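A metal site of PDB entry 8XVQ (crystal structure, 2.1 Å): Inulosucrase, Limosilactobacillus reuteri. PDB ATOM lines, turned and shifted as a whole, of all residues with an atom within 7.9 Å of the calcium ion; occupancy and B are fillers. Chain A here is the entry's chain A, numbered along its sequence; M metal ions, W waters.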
ATOM      1  N   GLN A 405      25.455 -22.533  -7.468  1.00  0.00           N
ATOM      2  CA  GLN A 405      25.184 -21.180  -7.952  1.00  0.00           C
ATOM      3  C   GLN A 405      26.404 -20.588  -8.653  1.00  0.00           C
ATOM      4  O   GLN A 405      27.534 -20.703  -8.173  1.00  0.00           O
ATOM      5  CB  GLN A 405      24.813 -20.263  -6.781  1.00  0.00           C
ATOM      6  CG  GLN A 405      24.178 -18.956  -7.188  1.00  0.00           C
ATOM      7  CD  GLN A 405      24.039 -17.978  -6.021  1.00  0.00           C
ATOM      8  OE1 GLN A 405      24.939 -17.856  -5.200  1.00  0.00           O
ATOM      9  NE2 GLN A 405      22.938 -17.244  -5.979  1.00  0.00           N
ATOM     10  N   TRP A 410      24.118 -15.143  -9.236  1.00  0.00           N
ATOM     11  CA  TRP A 410      24.148 -14.257  -8.075  1.00  0.00           C
ATOM     12  C   TRP A 410      24.036 -12.777  -8.490  1.00  0.00           C
ATOM     13  O   TRP A 410      23.304 -12.007  -7.883  1.00  0.00           O
ATOM     14  CB  TRP A 410      25.427 -14.477  -7.261  1.00  0.00           C
ATOM     15  CG  TRP A 410      25.647 -13.463  -6.186  1.00  0.00           C
ATOM     16  CD1 TRP A 410      25.101 -13.450  -4.934  1.00  0.00           C
ATOM     17  CD2 TRP A 410      26.494 -12.298  -6.268  1.00  0.00           C
ATOM     18  NE1 TRP A 410      25.545 -12.358  -4.238  1.00  0.00           N
ATOM     19  CE2 TRP A 410      26.397 -11.626  -5.032  1.00  0.00           C
ATOM     20  CE3 TRP A 410      27.307 -11.767  -7.264  1.00  0.00           C
ATOM     21  CZ2 TRP A 410      27.099 -10.457  -4.759  1.00  0.00           C
ATOM     22  CZ3 TRP A 410      28.001 -10.588  -6.996  1.00  0.00           C
ATOM     23  CH2 TRP A 410      27.896  -9.955  -5.754  1.00  0.00           C
ATOM     24  N   ALA A 417      21.291  -8.766  -0.391  1.00  0.00           N
ATOM     25  CA  ALA A 417      20.847  -9.725   0.605  1.00  0.00           C
ATOM     26  C   ALA A 417      21.383 -11.131   0.351  1.00  0.00           C
ATOM     27  O   ALA A 417      21.198 -12.008   1.175  1.00  0.00           O
ATOM     28  CB  ALA A 417      19.325  -9.757   0.660  1.00  0.00           C
ATOM     29  N   ASP A 418      22.071 -11.338  -0.768  1.00  0.00           N
ATOM     30  CA  ASP A 418      22.480 -12.668  -1.159  1.00  0.00           C
ATOM     31  C   ASP A 418      23.981 -12.800  -1.062  1.00  0.00           C
ATOM     32  O   ASP A 418      24.728 -11.961  -1.540  1.00  0.00           O
ATOM     33  CB  ASP A 418      22.037 -12.973  -2.576  1.00  0.00           C
ATOM     34  CG  ASP A 418      22.085 -14.467  -2.903  1.00  0.00           C
ATOM     35  OD1 ASP A 418      22.086 -15.292  -1.973  1.00  0.00           O
ATOM     36  OD2 ASP A 418      22.126 -14.803  -4.099  1.00  0.00           O
ATOM     37  N   ASN A 419      24.409 -13.885  -0.417  1.00  0.00           N
ATOM     38  CA  ASN A 419      25.801 -14.211  -0.297  1.00  0.00           C
ATOM     39  C   ASN A 419      26.271 -14.854  -1.598  1.00  0.00           C
ATOM     40  O   ASN A 419      25.465 -15.343  -2.391  1.00  0.00           O
ATOM     41  CB  ASN A 419      25.993 -15.164   0.878  1.00  0.00           C
ATOM     42  CG  ASN A 419      27.425 -15.205   1.400  1.00  0.00           C
ATOM     43  OD1 ASN A 419      28.257 -14.324   1.115  1.00  0.00           O
ATOM     44  ND2 ASN A 419      27.717 -16.244   2.179  1.00  0.00           N
ATOM     45  N   ILE A 420      27.575 -14.807  -1.809  1.00  0.00           N
ATOM     46  CA  ILE A 420      28.196 -15.441  -2.960  1.00  0.00           C
ATOM     47  C   ILE A 420      29.374 -16.253  -2.432  1.00  0.00           C
ATOM     48  O   ILE A 420      30.200 -15.732  -1.685  1.00  0.00           O
ATOM     49  CB  ILE A 420      28.665 -14.434  -4.040  1.00  0.00           C
ATOM     50  CG1 ILE A 420      29.502 -15.174  -5.079  1.00  0.00           C
ATOM     51  CG2 ILE A 420      29.445 -13.273  -3.427  1.00  0.00           C
ATOM     52  CD1 ILE A 420      29.958 -14.324  -6.221  1.00  0.00           C
ATOM     53  N   ALA A 421      29.437 -17.523  -2.813  1.00  0.00           N
ATOM     54  CA  ALA A 421      30.444 -18.413  -2.248  1.00  0.00           C
ATOM     55  C   ALA A 421      30.823 -19.484  -3.268  1.00  0.00           C
ATOM     56  O   ALA A 421      29.949 -20.136  -3.840  1.00  0.00           O
ATOM     57  CB  ALA A 421      29.966 -19.054  -0.965  1.00  0.00           C
ATOM     58  N   ALA A 441      29.846 -23.538  -1.303  1.00  0.00           N
ATOM     59  CA  ALA A 441      29.072 -22.961  -2.394  1.00  0.00           C
ATOM     60  C   ALA A 441      27.636 -22.650  -1.943  1.00  0.00           C
ATOM     61  O   ALA A 441      27.325 -22.756  -0.771  1.00  0.00           O
ATOM     62  CB  ALA A 441      29.060 -23.916  -3.583  1.00  0.00           C
ATOM     63  N   SER A 442      26.796 -22.227  -2.889  1.00  0.00           N
ATOM     64  CA  SER A 442      25.355 -22.176  -2.665  1.00  0.00           C
ATOM     65  C   SER A 442      24.690 -23.129  -3.638  1.00  0.00           C
ATOM     66  O   SER A 442      25.260 -23.426  -4.681  1.00  0.00           O
ATOM     67  CB  SER A 442      24.847 -20.763  -2.903  1.00  0.00           C
ATOM     68  OG  SER A 442      25.602 -19.848  -2.130  1.00  0.00           O
ATOM     69  N   THR A 443      23.506 -23.627  -3.309  1.00  0.00           N
ATOM     70  CA  THR A 443      22.777 -24.477  -4.274  1.00  0.00           C
ATOM     71  C   THR A 443      22.439 -23.680  -5.569  1.00  0.00           C
ATOM     72  O   THR A 443      22.300 -22.450  -5.564  1.00  0.00           O
ATOM     73  CB  THR A 443      21.432 -25.028  -3.739  1.00  0.00           C
ATOM     74  OG1 THR A 443      20.520 -23.935  -3.524  1.00  0.00           O
ATOM     75  CG2 THR A 443      21.616 -25.816  -2.472  1.00  0.00           C
ATOM     76  N   TYR A 448      16.902 -24.263  -5.563  1.00  0.00           N
ATOM     77  CA  TYR A 448      17.406 -22.901  -5.468  1.00  0.00           C
ATOM     78  C   TYR A 448      16.799 -22.099  -4.330  1.00  0.00           C
ATOM     79  O   TYR A 448      15.692 -22.370  -3.854  1.00  0.00           O
ATOM     80  CB  TYR A 448      17.207 -22.167  -6.804  1.00  0.00           C
ATOM     81  CG  TYR A 448      18.153 -21.007  -7.060  1.00  0.00           C
ATOM     82  CD1 TYR A 448      19.525 -21.123  -6.822  1.00  0.00           C
ATOM     83  CD2 TYR A 448      17.682 -19.785  -7.572  1.00  0.00           C
ATOM     84  CE1 TYR A 448      20.399 -20.082  -7.097  1.00  0.00           C
ATOM     85  CE2 TYR A 448      18.540 -18.724  -7.832  1.00  0.00           C
ATOM     86  CZ  TYR A 448      19.893 -18.865  -7.601  1.00  0.00           C
ATOM     87  OH  TYR A 448      20.760 -17.820  -7.849  1.00  0.00           O
ATOM     88  N   GLN A 449      17.539 -21.114  -3.871  1.00  0.00           N
ATOM     89  CA  GLN A 449      17.011 -20.129  -2.948  1.00  0.00           C
ATOM     90  C   GLN A 449      15.749 -19.469  -3.507  1.00  0.00           C
ATOM     91  O   GLN A 449      15.572 -19.375  -4.715  1.00  0.00           O
ATOM     92  CB  GLN A 449      18.045 -19.052  -2.698  1.00  0.00           C
ATOM     93  CG  GLN A 449      18.369 -18.226  -3.944  1.00  0.00           C
ATOM     94  CD  GLN A 449      19.631 -17.406  -3.794  1.00  0.00           C
ATOM     95  OE1 GLN A 449      20.467 -17.689  -2.950  1.00  0.00           O
ATOM     96  NE2 GLN A 449      19.779 -16.377  -4.627  1.00  0.00           N
ATOM     97  N   GLY A 450      14.883 -19.003  -2.617  1.00  0.00           N
ATOM     98  CA  GLY A 450      13.734 -18.202  -3.010  1.00  0.00           C
ATOM     99  C   GLY A 450      12.691 -18.205  -1.906  1.00  0.00           C
ATOM    100  O   GLY A 450      12.761 -19.023  -0.967  1.00  0.00           O
ATOM    101  N   ARG A 483      16.077 -13.254   4.967  1.00  0.00           N
ATOM    102  CA  ARG A 483      17.169 -14.241   5.112  1.00  0.00           C
ATOM    103  C   ARG A 483      16.731 -15.615   4.642  1.00  0.00           C
ATOM    104  O   ARG A 483      17.459 -16.277   3.918  1.00  0.00           O
ATOM    105  CB  ARG A 483      17.660 -14.325   6.556  1.00  0.00           C
ATOM    106  CG  ARG A 483      18.492 -13.135   6.955  1.00  0.00           C
ATOM    107  CD  ARG A 483      18.624 -13.015   8.460  1.00  0.00           C
ATOM    108  NE  ARG A 483      19.452 -11.867   8.852  1.00  0.00           N
ATOM    109  CZ  ARG A 483      20.737 -11.934   9.192  1.00  0.00           C
ATOM    110  NH1 ARG A 483      21.398 -13.100   9.229  1.00  0.00           N
ATOM    111  NH2 ARG A 483      21.393 -10.829   9.502  1.00  0.00           N
ATOM    112  N   ALA A 484      15.525 -16.024   5.030  1.00  0.00           N
ATOM    113  CA  ALA A 484      14.983 -17.314   4.592  1.00  0.00           C
ATOM    114  C   ALA A 484      14.837 -17.444   3.063  1.00  0.00           C
ATOM    115  O   ALA A 484      15.039 -18.532   2.475  1.00  0.00           O
ATOM    116  CB  ALA A 484      13.648 -17.560   5.249  1.00  0.00           C
ATOM    117  N   THR A 485      14.428 -16.324   2.453  1.00  0.00           N
ATOM    118  CA  THR A 485      14.272 -16.186   1.012  1.00  0.00           C
ATOM    119  C   THR A 485      15.597 -16.318   0.275  1.00  0.00           C
ATOM    120  O   THR A 485      15.643 -16.883  -0.794  1.00  0.00           O
ATOM    121  CB  THR A 485      13.652 -14.807   0.670  1.00  0.00           C
ATOM    122  OG1 THR A 485      12.321 -14.750   1.189  1.00  0.00           O
ATOM    123  CG2 THR A 485      13.626 -14.547  -0.835  1.00  0.00           C
ATOM    124  N   TRP A 486      16.667 -15.834   0.878  1.00  0.00           N
ATOM    125  CA  TRP A 486      17.978 -15.864   0.252  1.00  0.00           C
ATOM    126  C   TRP A 486      18.944 -17.005   0.728  1.00  0.00           C
ATOM    127  O   TRP A 486      20.008 -17.181   0.148  1.00  0.00           O
ATOM    128  CB  TRP A 486      18.631 -14.493   0.407  1.00  0.00           C
ATOM    129  CG  TRP A 486      17.911 -13.383  -0.371  1.00  0.00           C
ATOM    130  CD1 TRP A 486      17.094 -12.417   0.146  1.00  0.00           C
ATOM    131  CD2 TRP A 486      17.950 -13.138  -1.797  1.00  0.00           C
ATOM    132  NE1 TRP A 486      16.642 -11.597  -0.848  1.00  0.00           N
ATOM    133  CE2 TRP A 486      17.146 -12.017  -2.049  1.00  0.00           C
ATOM    134  CE3 TRP A 486      18.615 -13.760  -2.873  1.00  0.00           C
ATOM    135  CZ2 TRP A 486      16.955 -11.484  -3.337  1.00  0.00           C
ATOM    136  CZ3 TRP A 486      18.431 -13.239  -4.156  1.00  0.00           C
ATOM    137  CH2 TRP A 486      17.607 -12.111  -4.377  1.00  0.00           C
ATOM    138  N   ALA A 487      18.564 -17.771   1.756  1.00  0.00           N
ATOM    139  CA  ALA A 487      19.466 -18.806   2.322  1.00  0.00           C
ATOM    140  C   ALA A 487      19.502 -20.082   1.467  1.00  0.00           C
ATOM    141  O   ALA A 487      18.472 -20.709   1.206  1.00  0.00           O
ATOM    142  CB  ALA A 487      19.065 -19.154   3.762  1.00  0.00           C
ATOM    143  N   ASN A 488      20.706 -20.478   1.076  1.00  0.00           N
ATOM    144  CA  ASN A 488      20.894 -21.763   0.373  1.00  0.00           C
ATOM    145  C   ASN A 488      22.361 -22.195   0.310  1.00  0.00           C
ATOM    146  O   ASN A 488      22.872 -22.631  -0.729  1.00  0.00           O
ATOM    147  CB  ASN A 488      20.331 -21.671  -1.039  1.00  0.00           C
ATOM    148  CG  ASN A 488      21.126 -20.728  -1.933  1.00  0.00           C
ATOM    149  OD1 ASN A 488      21.721 -19.750  -1.466  1.00  0.00           O
ATOM    150  ND2 ASN A 488      21.147 -21.036  -3.236  1.00  0.00           N
ATOM    151  N   ALA A 489      23.032 -22.086   1.453  1.00  0.00           N
ATOM    152  CA  ALA A 489      24.406 -22.537   1.562  1.00  0.00           C
ATOM    153  C   ALA A 489      24.523 -24.026   1.244  1.00  0.00           C
ATOM    154  O   ALA A 489      23.629 -24.808   1.547  1.00  0.00           O
ATOM    155  CB  ALA A 489      24.936 -22.262   2.956  1.00  0.00           C
ATOM    156  N   SER A 519      20.536 -21.119   6.287  1.00  0.00           N
ATOM    157  CA  SER A 519      21.775 -20.352   6.338  1.00  0.00           C
ATOM    158  C   SER A 519      22.342 -20.116   4.940  1.00  0.00           C
ATOM    159  O   SER A 519      22.213 -20.961   4.049  1.00  0.00           O
ATOM    160  CB  SER A 519      22.829 -21.080   7.175  1.00  0.00           C
ATOM    161  OG  SER A 519      24.042 -20.310   7.211  1.00  0.00           O
ATOM    162  N   ASP A 520      22.993 -18.960   4.763  1.00  0.00           N
ATOM    163  CA  ASP A 520      23.648 -18.662   3.510  1.00  0.00           C
ATOM    164  C   ASP A 520      25.174 -18.666   3.641  1.00  0.00           C
ATOM    165  O   ASP A 520      25.873 -18.184   2.751  1.00  0.00           O
ATOM    166  CB  ASP A 520      23.135 -17.309   2.948  1.00  0.00           C
ATOM    167  CG  ASP A 520      22.895 -17.314   1.423  1.00  0.00           C
ATOM    168  OD1 ASP A 520      22.735 -18.397   0.800  1.00  0.00           O
ATOM    169  OD2 ASP A 520      22.827 -16.187   0.849  1.00  0.00           O
ATOM    170  N   GLU A 521      25.724 -19.242   4.719  1.00  0.00           N
ATOM    171  CA  GLU A 521      27.195 -19.386   4.818  1.00  0.00           C
ATOM    172  C   GLU A 521      27.647 -20.484   5.769  1.00  0.00           C
ATOM    173  O   GLU A 521      27.464 -20.400   6.990  1.00  0.00           O
ATOM    174  CB  GLU A 521      27.831 -18.070   5.246  1.00  0.00           C
ATOM    175  CG  GLU A 521      29.320 -18.011   4.984  1.00  0.00           C
ATOM    176  CD  GLU A 521      29.869 -16.622   5.264  1.00  0.00           C
ATOM    177  OE1 GLU A 521      30.063 -16.318   6.468  1.00  0.00           O
ATOM    178  OE2 GLU A 521      30.095 -15.861   4.294  1.00  0.00           O
HETATM  179 CA    CA M   1      21.894 -17.453  -1.167  1.00  0.00          CA
HETATM  180  O   HOH W   1      23.933 -17.521  -2.316  1.00  0.00           O
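The calcium ion is bound by OE1 of Gln 449, O of Trp 486, OD1 of Asp 418, OD1 of Asn 488, OD1 of Asp 520, water W1 and OD2 of Asp 520.
Five residues have an atom within 4 Å of the calcium ion: Asp 418, Gln 449, Trp 486, Asn 488 and Asp 520. The nearest printed residue that does not touch the calcium ion is Asn 419 (4.3 Å).
Water W1 lies within hydrogen-bond range of O of Asn 419, OG of Ser 442 and OE1 of Gln 405.
OD2 of Asp 418 is in hydrogen-bond range of NE2 of Gln 405, 3.2 Å away. O of Asp 418 is in hydrogen-bond range of NE1 of Trp 410 (2.8 Å). N of Asn 488 sits at hydrogen-bond distance from O of Ser 519 (3.4 Å). The backbone carbonyl oxygen (O) of Asn 488 sits at hydrogen-bond distance from the backbone NH (N) of Thr 443, at 2.8 Å. The backbone carbonyl oxygen of Asp 520 lies within hydrogen-bond range of the side-chain amide nitrogen of Asn 419 (2.7 Å).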
